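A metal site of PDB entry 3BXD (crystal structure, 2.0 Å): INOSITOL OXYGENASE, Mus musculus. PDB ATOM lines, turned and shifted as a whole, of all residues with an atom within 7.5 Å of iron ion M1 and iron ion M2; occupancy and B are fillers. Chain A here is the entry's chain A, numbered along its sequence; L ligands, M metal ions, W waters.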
ATOM      1  N   ASP A  89     -18.233  15.293 -24.927  1.00  0.00           N
ATOM      2  CA  ASP A  89     -18.722  16.459 -24.187  1.00  0.00           C
ATOM      3  C   ASP A  89     -18.941  16.105 -22.706  1.00  0.00           C
ATOM      4  O   ASP A  89     -19.671  15.163 -22.381  1.00  0.00           O
ATOM      5  CB  ASP A  89     -20.002  16.974 -24.851  1.00  0.00           C
ATOM      6  CG  ASP A  89     -20.467  18.282 -24.265  1.00  0.00           C
ATOM      7  OD1 ASP A  89     -20.260  18.495 -23.056  1.00  0.00           O
ATOM      8  OD2 ASP A  89     -21.055  19.095 -25.016  1.00  0.00           O
ATOM      9  N   ASP A  92     -22.632  16.945 -20.943  1.00  0.00           N
ATOM     10  CA  ASP A  92     -23.823  16.243 -21.409  1.00  0.00           C
ATOM     11  C   ASP A  92     -24.065  14.966 -20.594  1.00  0.00           C
ATOM     12  O   ASP A  92     -23.242  14.058 -20.606  1.00  0.00           O
ATOM     13  CB  ASP A  92     -23.669  15.895 -22.893  1.00  0.00           C
ATOM     14  CG  ASP A  92     -25.004  15.772 -23.616  1.00  0.00           C
ATOM     15  OD1 ASP A  92     -26.066  15.720 -22.957  1.00  0.00           O
ATOM     16  OD2 ASP A  92     -24.990  15.728 -24.870  1.00  0.00           O
ATOM     17  N   ASN A  99     -18.495  13.332 -30.339  1.00  0.00           N
ATOM     18  CA  ASN A  99     -19.572  14.282 -30.574  1.00  0.00           C
ATOM     19  C   ASN A  99     -19.885  14.402 -32.051  1.00  0.00           C
ATOM     20  O   ASN A  99     -20.942  14.916 -32.429  1.00  0.00           O
ATOM     21  CB  ASN A  99     -19.195  15.646 -29.992  1.00  0.00           C
ATOM     22  CG  ASN A  99     -20.412  16.489 -29.643  1.00  0.00           C
ATOM     23  OD1 ASN A  99     -21.103  16.211 -28.659  1.00  0.00           O
ATOM     24  ND2 ASN A  99     -20.686  17.510 -30.454  1.00  0.00           N
ATOM     25  N   HIS A 102     -23.053  12.647 -32.774  1.00  0.00           N
ATOM     26  CA  HIS A 102     -24.201  13.431 -32.344  1.00  0.00           C
ATOM     27  C   HIS A 102     -24.600  14.452 -33.410  1.00  0.00           C
ATOM     28  O   HIS A 102     -25.790  14.718 -33.599  1.00  0.00           O
ATOM     29  CB  HIS A 102     -23.907  14.156 -31.029  1.00  0.00           C
ATOM     30  CG  HIS A 102     -24.769  15.359 -30.797  1.00  0.00           C
ATOM     31  ND1 HIS A 102     -26.052  15.268 -30.284  1.00  0.00           N
ATOM     32  CD2 HIS A 102     -24.543  16.677 -31.006  1.00  0.00           C
ATOM     33  CE1 HIS A 102     -26.572  16.471 -30.200  1.00  0.00           C
ATOM     34  NE2 HIS A 102     -25.680  17.349 -30.629  1.00  0.00           N
ATOM     35  N   ALA A 103     -23.620  15.011 -34.103  1.00  0.00           N
ATOM     36  CA  ALA A 103     -23.893  15.934 -35.194  1.00  0.00           C
ATOM     37  C   ALA A 103     -24.777  15.263 -36.270  1.00  0.00           C
ATOM     38  O   ALA A 103     -25.756  15.857 -36.736  1.00  0.00           O
ATOM     39  CB  ALA A 103     -22.597  16.433 -35.802  1.00  0.00           C
ATOM     40  N   THR A 106     -28.398  14.474 -35.076  1.00  0.00           N
ATOM     41  CA  THR A 106     -29.243  15.650 -34.971  1.00  0.00           C
ATOM     42  C   THR A 106     -29.713  16.065 -36.360  1.00  0.00           C
ATOM     43  O   THR A 106     -30.888  16.351 -36.577  1.00  0.00           O
ATOM     44  CB  THR A 106     -28.517  16.836 -34.295  1.00  0.00           C
ATOM     45  OG1 THR A 106     -28.154  16.478 -32.947  1.00  0.00           O
ATOM     46  CG2 THR A 106     -29.407  18.064 -34.256  1.00  0.00           C
ATOM     47  N   GLY A 124     -28.395  21.157 -38.110  1.00  0.00           N
ATOM     48  CA  GLY A 124     -28.185  20.012 -37.220  1.00  0.00           C
ATOM     49  C   GLY A 124     -26.751  19.513 -37.200  1.00  0.00           C
ATOM     50  O   GLY A 124     -26.159  19.296 -36.145  1.00  0.00           O
ATOM     51  N   HIS A 127     -24.263  22.577 -35.762  1.00  0.00           N
ATOM     52  CA  HIS A 127     -24.538  23.392 -34.560  1.00  0.00           C
ATOM     53  C   HIS A 127     -23.495  23.289 -33.450  1.00  0.00           C
ATOM     54  O   HIS A 127     -23.289  24.256 -32.698  1.00  0.00           O
ATOM     55  CB  HIS A 127     -25.925  23.063 -34.008  1.00  0.00           C
ATOM     56  CG  HIS A 127     -25.984  21.788 -33.231  1.00  0.00           C
ATOM     57  ND1 HIS A 127     -26.155  20.563 -33.840  1.00  0.00           N
ATOM     58  CD2 HIS A 127     -25.894  21.545 -31.902  1.00  0.00           C
ATOM     59  CE1 HIS A 127     -26.160  19.619 -32.921  1.00  0.00           C
ATOM     60  NE2 HIS A 127     -25.997  20.197 -31.732  1.00  0.00           N
ATOM     61  N   ASP A 128     -22.830  22.147 -33.341  1.00  0.00           N
ATOM     62  CA  ASP A 128     -21.862  21.936 -32.269  1.00  0.00           C
ATOM     63  C   ASP A 128     -20.394  21.961 -32.712  1.00  0.00           C
ATOM     64  O   ASP A 128     -19.522  21.507 -31.964  1.00  0.00           O
ATOM     65  CB  ASP A 128     -22.131  20.597 -31.579  1.00  0.00           C
ATOM     66  CG  ASP A 128     -23.172  20.711 -30.491  1.00  0.00           C
ATOM     67  OD1 ASP A 128     -23.517  21.855 -30.127  1.00  0.00           O
ATOM     68  OD2 ASP A 128     -23.627  19.662 -30.002  1.00  0.00           O
ATOM     69  N   LEU A 129     -20.128  22.499 -33.892  1.00  0.00           N
ATOM     70  CA  LEU A 129     -18.778  22.461 -34.432  1.00  0.00           C
ATOM     71  C   LEU A 129     -17.830  23.401 -33.669  1.00  0.00           C
ATOM     72  O   LEU A 129     -16.610  23.272 -33.752  1.00  0.00           O
ATOM     73  CB  LEU A 129     -18.786  22.784 -35.925  1.00  0.00           C
ATOM     74  CG  LEU A 129     -19.451  21.696 -36.801  1.00  0.00           C
ATOM     75  CD1 LEU A 129     -19.428  22.073 -38.274  1.00  0.00           C
ATOM     76  CD2 LEU A 129     -18.765  20.354 -36.600  1.00  0.00           C
ATOM     77  N   LYS A 131     -17.199  23.337 -30.702  1.00  0.00           N
ATOM     78  CA  LYS A 131     -16.516  22.575 -29.645  1.00  0.00           C
ATOM     79  C   LYS A 131     -15.116  22.135 -30.055  1.00  0.00           C
ATOM     80  O   LYS A 131     -14.420  21.484 -29.276  1.00  0.00           O
ATOM     81  CB  LYS A 131     -17.332  21.337 -29.276  1.00  0.00           C
ATOM     82  CG  LYS A 131     -18.671  21.650 -28.658  1.00  0.00           C
ATOM     83  CD  LYS A 131     -19.528  20.417 -28.548  1.00  0.00           C
ATOM     84  CE  LYS A 131     -20.879  20.739 -27.949  1.00  0.00           C
ATOM     85  NZ  LYS A 131     -21.724  19.523 -27.900  1.00  0.00           N
ATOM     86  N   VAL A 143     -16.225  25.939 -23.273  1.00  0.00           N
ATOM     87  CA  VAL A 143     -16.500  25.446 -24.624  1.00  0.00           C
ATOM     88  C   VAL A 143     -17.905  24.863 -24.753  1.00  0.00           C
ATOM     89  O   VAL A 143     -18.650  25.196 -25.676  1.00  0.00           O
ATOM     90  CB  VAL A 143     -15.484  24.364 -25.027  1.00  0.00           C
ATOM     91  CG1 VAL A 143     -15.869  23.747 -26.363  1.00  0.00           C
ATOM     92  CG2 VAL A 143     -14.090  24.942 -25.101  1.00  0.00           C
ATOM     93  N   VAL A 144     -18.265  23.986 -23.821  1.00  0.00           N
ATOM     94  CA  VAL A 144     -19.531  23.282 -23.852  1.00  0.00           C
ATOM     95  C   VAL A 144     -20.447  23.710 -22.709  1.00  0.00           C
ATOM     96  O   VAL A 144     -20.058  24.482 -21.831  1.00  0.00           O
ATOM     97  CB  VAL A 144     -19.311  21.758 -23.731  1.00  0.00           C
ATOM     98  CG1 VAL A 144     -18.378  21.264 -24.815  1.00  0.00           C
ATOM     99  CG2 VAL A 144     -18.765  21.404 -22.357  1.00  0.00           C
ATOM    100  N   GLY A 145     -21.678  23.198 -22.749  1.00  0.00           N
ATOM    101  CA  GLY A 145     -22.617  23.359 -21.655  1.00  0.00           C
ATOM    102  C   GLY A 145     -23.680  24.402 -21.896  1.00  0.00           C
ATOM    103  O   GLY A 145     -23.624  25.176 -22.853  1.00  0.00           O
ATOM    104  N   HIS A 198     -19.298  27.306 -27.498  1.00  0.00           N
ATOM    105  CA  HIS A 198     -19.441  26.938 -28.901  1.00  0.00           C
ATOM    106  C   HIS A 198     -20.538  27.692 -29.643  1.00  0.00           C
ATOM    107  O   HIS A 198     -20.439  27.882 -30.857  1.00  0.00           O
ATOM    108  CB  HIS A 198     -19.664  25.430 -29.014  1.00  0.00           C
ATOM    109  CG  HIS A 198     -20.928  24.948 -28.364  1.00  0.00           C
ATOM    110  ND1 HIS A 198     -21.146  25.039 -27.012  1.00  0.00           N
ATOM    111  CD2 HIS A 198     -22.017  24.337 -28.881  1.00  0.00           C
ATOM    112  CE1 HIS A 198     -22.320  24.519 -26.724  1.00  0.00           C
ATOM    113  NE2 HIS A 198     -22.878  24.085 -27.846  1.00  0.00           N
ATOM    114  N   ASP A 199     -21.567  28.142 -28.917  1.00  0.00           N
ATOM    115  CA  ASP A 199     -22.691  28.850 -29.534  1.00  0.00           C
ATOM    116  C   ASP A 199     -22.204  30.104 -30.203  1.00  0.00           C
ATOM    117  O   ASP A 199     -22.332  30.265 -31.412  1.00  0.00           O
ATOM    118  CB  ASP A 199     -23.730  29.284 -28.502  1.00  0.00           C
ATOM    119  CG  ASP A 199     -24.609  28.163 -28.028  1.00  0.00           C
ATOM    120  OD1 ASP A 199     -24.129  27.012 -28.026  1.00  0.00           O
ATOM    121  OD2 ASP A 199     -25.772  28.439 -27.660  1.00  0.00           O
ATOM    122  N   ILE A 221     -28.441  28.574 -33.765  1.00  0.00           N
ATOM    123  CA  ILE A 221     -27.122  28.110 -33.362  1.00  0.00           C
ATOM    124  C   ILE A 221     -26.579  28.978 -32.238  1.00  0.00           C
ATOM    125  O   ILE A 221     -26.017  28.471 -31.256  1.00  0.00           O
ATOM    126  CB  ILE A 221     -26.165  28.115 -34.566  1.00  0.00           C
ATOM    127  CG1 ILE A 221     -26.518  26.961 -35.503  1.00  0.00           C
ATOM    128  CG2 ILE A 221     -24.724  28.016 -34.126  1.00  0.00           C
ATOM    129  CD1 ILE A 221     -25.782  27.002 -36.815  1.00  0.00           C
ATOM    130  N   HIS A 224     -28.762  28.090 -28.972  1.00  0.00           N
ATOM    131  CA  HIS A 224     -29.309  26.747 -28.772  1.00  0.00           C
ATOM    132  C   HIS A 224     -28.945  26.162 -27.403  1.00  0.00           C
ATOM    133  O   HIS A 224     -29.624  25.258 -26.913  1.00  0.00           O
ATOM    134  CB  HIS A 224     -28.857  25.795 -29.889  1.00  0.00           C
ATOM    135  CG  HIS A 224     -27.469  25.262 -29.708  1.00  0.00           C
ATOM    136  ND1 HIS A 224     -26.355  25.881 -30.236  1.00  0.00           N
ATOM    137  CD2 HIS A 224     -27.009  24.169 -29.050  1.00  0.00           C
ATOM    138  CE1 HIS A 224     -25.279  25.188 -29.926  1.00  0.00           C
ATOM    139  NE2 HIS A 224     -25.654  24.147 -29.189  1.00  0.00           N
ATOM    140  N   SER A 225     -27.903  26.691 -26.795  1.00  0.00           N
ATOM    141  CA  SER A 225     -27.457  26.236 -25.474  1.00  0.00           C
ATOM    142  C   SER A 225     -28.129  27.000 -24.334  1.00  0.00           C
ATOM    143  O   SER A 225     -27.944  26.664 -23.168  1.00  0.00           O
ATOM    144  CB  SER A 225     -25.946  26.403 -25.354  1.00  0.00           C
ATOM    145  OG  SER A 225     -25.256  25.739 -26.403  1.00  0.00           O
ATOM    146  N   TYR A 227     -30.583  27.313 -22.321  1.00  0.00           N
ATOM    147  CA  TYR A 227     -31.717  26.586 -21.802  1.00  0.00           C
ATOM    148  C   TYR A 227     -32.570  27.424 -20.861  1.00  0.00           C
ATOM    149  O   TYR A 227     -33.783  27.427 -20.987  1.00  0.00           O
ATOM    150  CB  TYR A 227     -31.272  25.300 -21.096  1.00  0.00           C
ATOM    151  CG  TYR A 227     -31.204  24.097 -22.014  1.00  0.00           C
ATOM    152  CD1 TYR A 227     -30.114  23.901 -22.869  1.00  0.00           C
ATOM    153  CD2 TYR A 227     -32.223  23.157 -22.032  1.00  0.00           C
ATOM    154  CE1 TYR A 227     -30.051  22.797 -23.705  1.00  0.00           C
ATOM    155  CE2 TYR A 227     -32.166  22.047 -22.872  1.00  0.00           C
ATOM    156  CZ  TYR A 227     -31.084  21.873 -23.700  1.00  0.00           C
ATOM    157  OH  TYR A 227     -31.013  20.775 -24.531  1.00  0.00           O
ATOM    158  N   PHE A 253     -35.623  23.285 -32.893  1.00  0.00           N
ATOM    159  CA  PHE A 253     -34.297  22.728 -33.059  1.00  0.00           C
ATOM    160  C   PHE A 253     -33.885  21.960 -31.820  1.00  0.00           C
ATOM    161  O   PHE A 253     -33.270  20.889 -31.907  1.00  0.00           O
ATOM    162  CB  PHE A 253     -33.255  23.806 -33.323  1.00  0.00           C
ATOM    163  CG  PHE A 253     -31.862  23.293 -33.244  1.00  0.00           C
ATOM    164  CD1 PHE A 253     -31.310  22.589 -34.297  1.00  0.00           C
ATOM    165  CD2 PHE A 253     -31.117  23.469 -32.100  1.00  0.00           C
ATOM    166  CE1 PHE A 253     -30.034  22.090 -34.213  1.00  0.00           C
ATOM    167  CE2 PHE A 253     -29.840  22.970 -32.016  1.00  0.00           C
ATOM    168  CZ  PHE A 253     -29.292  22.290 -33.071  1.00  0.00           C
ATOM    169  N   PHE A 256     -34.808  18.167 -31.290  1.00  0.00           N
ATOM    170  CA  PHE A 256     -34.002  17.240 -32.086  1.00  0.00           C
ATOM    171  C   PHE A 256     -32.586  17.196 -31.545  1.00  0.00           C
ATOM    172  O   PHE A 256     -31.923  16.165 -31.601  1.00  0.00           O
ATOM    173  CB  PHE A 256     -33.939  17.685 -33.555  1.00  0.00           C
ATOM    174  CG  PHE A 256     -35.273  17.727 -34.245  1.00  0.00           C
ATOM    175  CD1 PHE A 256     -35.918  16.553 -34.610  1.00  0.00           C
ATOM    176  CD2 PHE A 256     -35.879  18.941 -34.539  1.00  0.00           C
ATOM    177  CE1 PHE A 256     -37.150  16.597 -35.235  1.00  0.00           C
ATOM    178  CE2 PHE A 256     -37.106  18.989 -35.178  1.00  0.00           C
ATOM    179  CZ  PHE A 256     -37.749  17.816 -35.525  1.00  0.00           C
ATOM    180  N   ASP A 257     -32.118  18.331 -31.034  1.00  0.00           N
ATOM    181  CA  ASP A 257     -30.763  18.439 -30.504  1.00  0.00           C
ATOM    182  C   ASP A 257     -30.647  17.463 -29.349  1.00  0.00           C
ATOM    183  O   ASP A 257     -29.696  16.709 -29.240  1.00  0.00           O
ATOM    184  CB  ASP A 257     -30.494  19.885 -30.043  1.00  0.00           C
ATOM    185  CG  ASP A 257     -29.116  20.068 -29.419  1.00  0.00           C
ATOM    186  OD1 ASP A 257     -28.224  19.229 -29.651  1.00  0.00           O
ATOM    187  OD2 ASP A 257     -28.926  21.075 -28.693  1.00  0.00           O
ATOM    188  N   LEU A 258     -31.681  17.467 -28.512  1.00  0.00           N
ATOM    189  CA  LEU A 258     -31.675  16.724 -27.261  1.00  0.00           C
ATOM    190  C   LEU A 258     -32.108  15.261 -27.445  1.00  0.00           C
ATOM    191  O   LEU A 258     -31.389  14.345 -27.035  1.00  0.00           O
ATOM    192  CB  LEU A 258     -32.601  17.431 -26.262  1.00  0.00           C
ATOM    193  CG  LEU A 258     -32.736  16.823 -24.877  1.00  0.00           C
ATOM    194  CD1 LEU A 258     -31.387  16.720 -24.199  1.00  0.00           C
ATOM    195  CD2 LEU A 258     -33.699  17.642 -24.033  1.00  0.00           C
ATOM    196  N   LYS A 261     -30.259  11.989 -29.218  1.00  0.00           N
ATOM    197  CA  LYS A 261     -29.085  11.405 -28.569  1.00  0.00           C
ATOM    198  C   LYS A 261     -29.325   9.933 -28.206  1.00  0.00           C
ATOM    199  O   LYS A 261     -30.200   9.628 -27.396  1.00  0.00           O
ATOM    200  CB  LYS A 261     -28.694  12.226 -27.329  1.00  0.00           C
ATOM    201  CG  LYS A 261     -28.049  13.572 -27.663  1.00  0.00           C
ATOM    202  CD  LYS A 261     -28.002  14.503 -26.456  1.00  0.00           C
ATOM    203  CE  LYS A 261     -27.468  15.877 -26.834  1.00  0.00           C
ATOM    204  NZ  LYS A 261     -27.567  16.869 -25.731  1.00  0.00           N
HETATM  205  O1  LIG L   1     -26.548  21.168 -28.471  1.00  0.00           O
HETATM  206  C1  LG2 L   2     -24.826  20.946 -26.024  1.00  0.00           C
HETATM  207  C2  LG2 L   2     -24.192  20.174 -24.856  1.00  0.00           C
HETATM  208  C3  LG2 L   2     -25.182  20.058 -23.705  1.00  0.00           C
HETATM  209  C4  LG2 L   2     -25.569  21.454 -23.244  1.00  0.00           C
HETATM  210  C5  LG2 L   2     -26.208  22.231 -24.389  1.00  0.00           C
HETATM  211  C6  LG2 L   2     -25.236  22.360 -25.550  1.00  0.00           C
HETATM  212  O1  LG2 L   2     -23.888  21.050 -27.080  1.00  0.00           O
HETATM  213  O2  LG2 L   2     -23.006  20.844 -24.409  1.00  0.00           O
HETATM  214  O3  LG2 L   2     -24.565  19.371 -22.621  1.00  0.00           O
HETATM  215  O4  LG2 L   2     -26.526  21.316 -22.205  1.00  0.00           O
HETATM  216  O5  LG2 L   2     -26.592  23.529 -23.915  1.00  0.00           O
HETATM  217  O6  LG2 L   2     -25.830  23.094 -26.619  1.00  0.00           O
HETATM  218 FE    FE M   1     -25.860  19.511 -29.719  1.00  0.00          FE
HETATM  219 FE    FE M   2     -24.596  22.498 -28.355  1.00  0.00          FE
HETATM  220  O   HOH W   1     -25.351  18.366 -27.826  1.00  0.00           O
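An oxygen (O2) of LG2 L2 lies within hydrogen-bond range of the side-chain carboxylate of Asp 89 (2.7 Å).
N of Gly 145 is in hydrogen-bond range of O2 of LG2 L2 (3.2 Å).
O1 of LG2 L2 sits close to NZ of Lys 131 (2.8 Å).
O of Ser 225 lies close to O5 of LG2 L2, at 3.5 Å.
An oxygen (O6) of LG2 L2 sits close to the side-chain hydroxyl of Ser 225, 2.7 Å away.
A ring nitrogen (NE2) of His 198 sits close to the side-chain carboxylate (OD1) of Asp 199, 3.2 Å away.
OG of Ser 225 lies close to NE2 of His 198 (3.2 Å).
The backbone carbonyl oxygen (O) of His 102 is in hydrogen-bond range of the side-chain hydroxyl (OG1) of Thr 106, 3.0 Å away.
ND1 of His 198 sits at hydrogen-bond distance from O of Val 143 (2.8 Å).
N of Ser 225 is in hydrogen-bond range of OD2 of Asp 199 (2.9 Å).
The backbone carbonyl oxygen (O) of Gly 124 sits at hydrogen-bond distance from a ring nitrogen (ND1) of His 127 (2.6 Å).
O of Ile 221 sits at hydrogen-bond distance from ND1 of His 224 (2.8 Å).
The side-chain carboxylate of Asp 128 sits close to the side-chain amino group of Lys 131 (2.8 Å).
Four residues have an atom within 4 Å of iron ion M1: His 102, His 127, Asp 128 and Asp 257.
OG of Ser 225 touches iron ion M2 (3.8 Å).
Of the 25 residues printed, 5 come within 4 Å of iron ion M2.
The nearest printed residue that does not touch iron ion M2 is Lys 131 (4.1 Å).
Iron ion M1 is bound by NE2 of His 127 (2.1 Å), O1 of LIG L1 (2.2 Å), OD2 of Asp 128 (2.3 Å), water W1 (2.3 Å), NE2 of His 102 (2.4 Å) and OD1 of Asp 257 (2.4 Å).
Iron ion M1 has six donor atoms within binding distance.
Iron ion M2 is bound by O1 of LG2 L2 (2.1 Å), NE2 of His 224 (2.1 Å), OD1 of Asp 128 (2.2 Å), O6 of LG2 L2 (2.2 Å), O1 of LIG L1 (2.4 Å) and NE2 of His 198 (2.4 Å).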
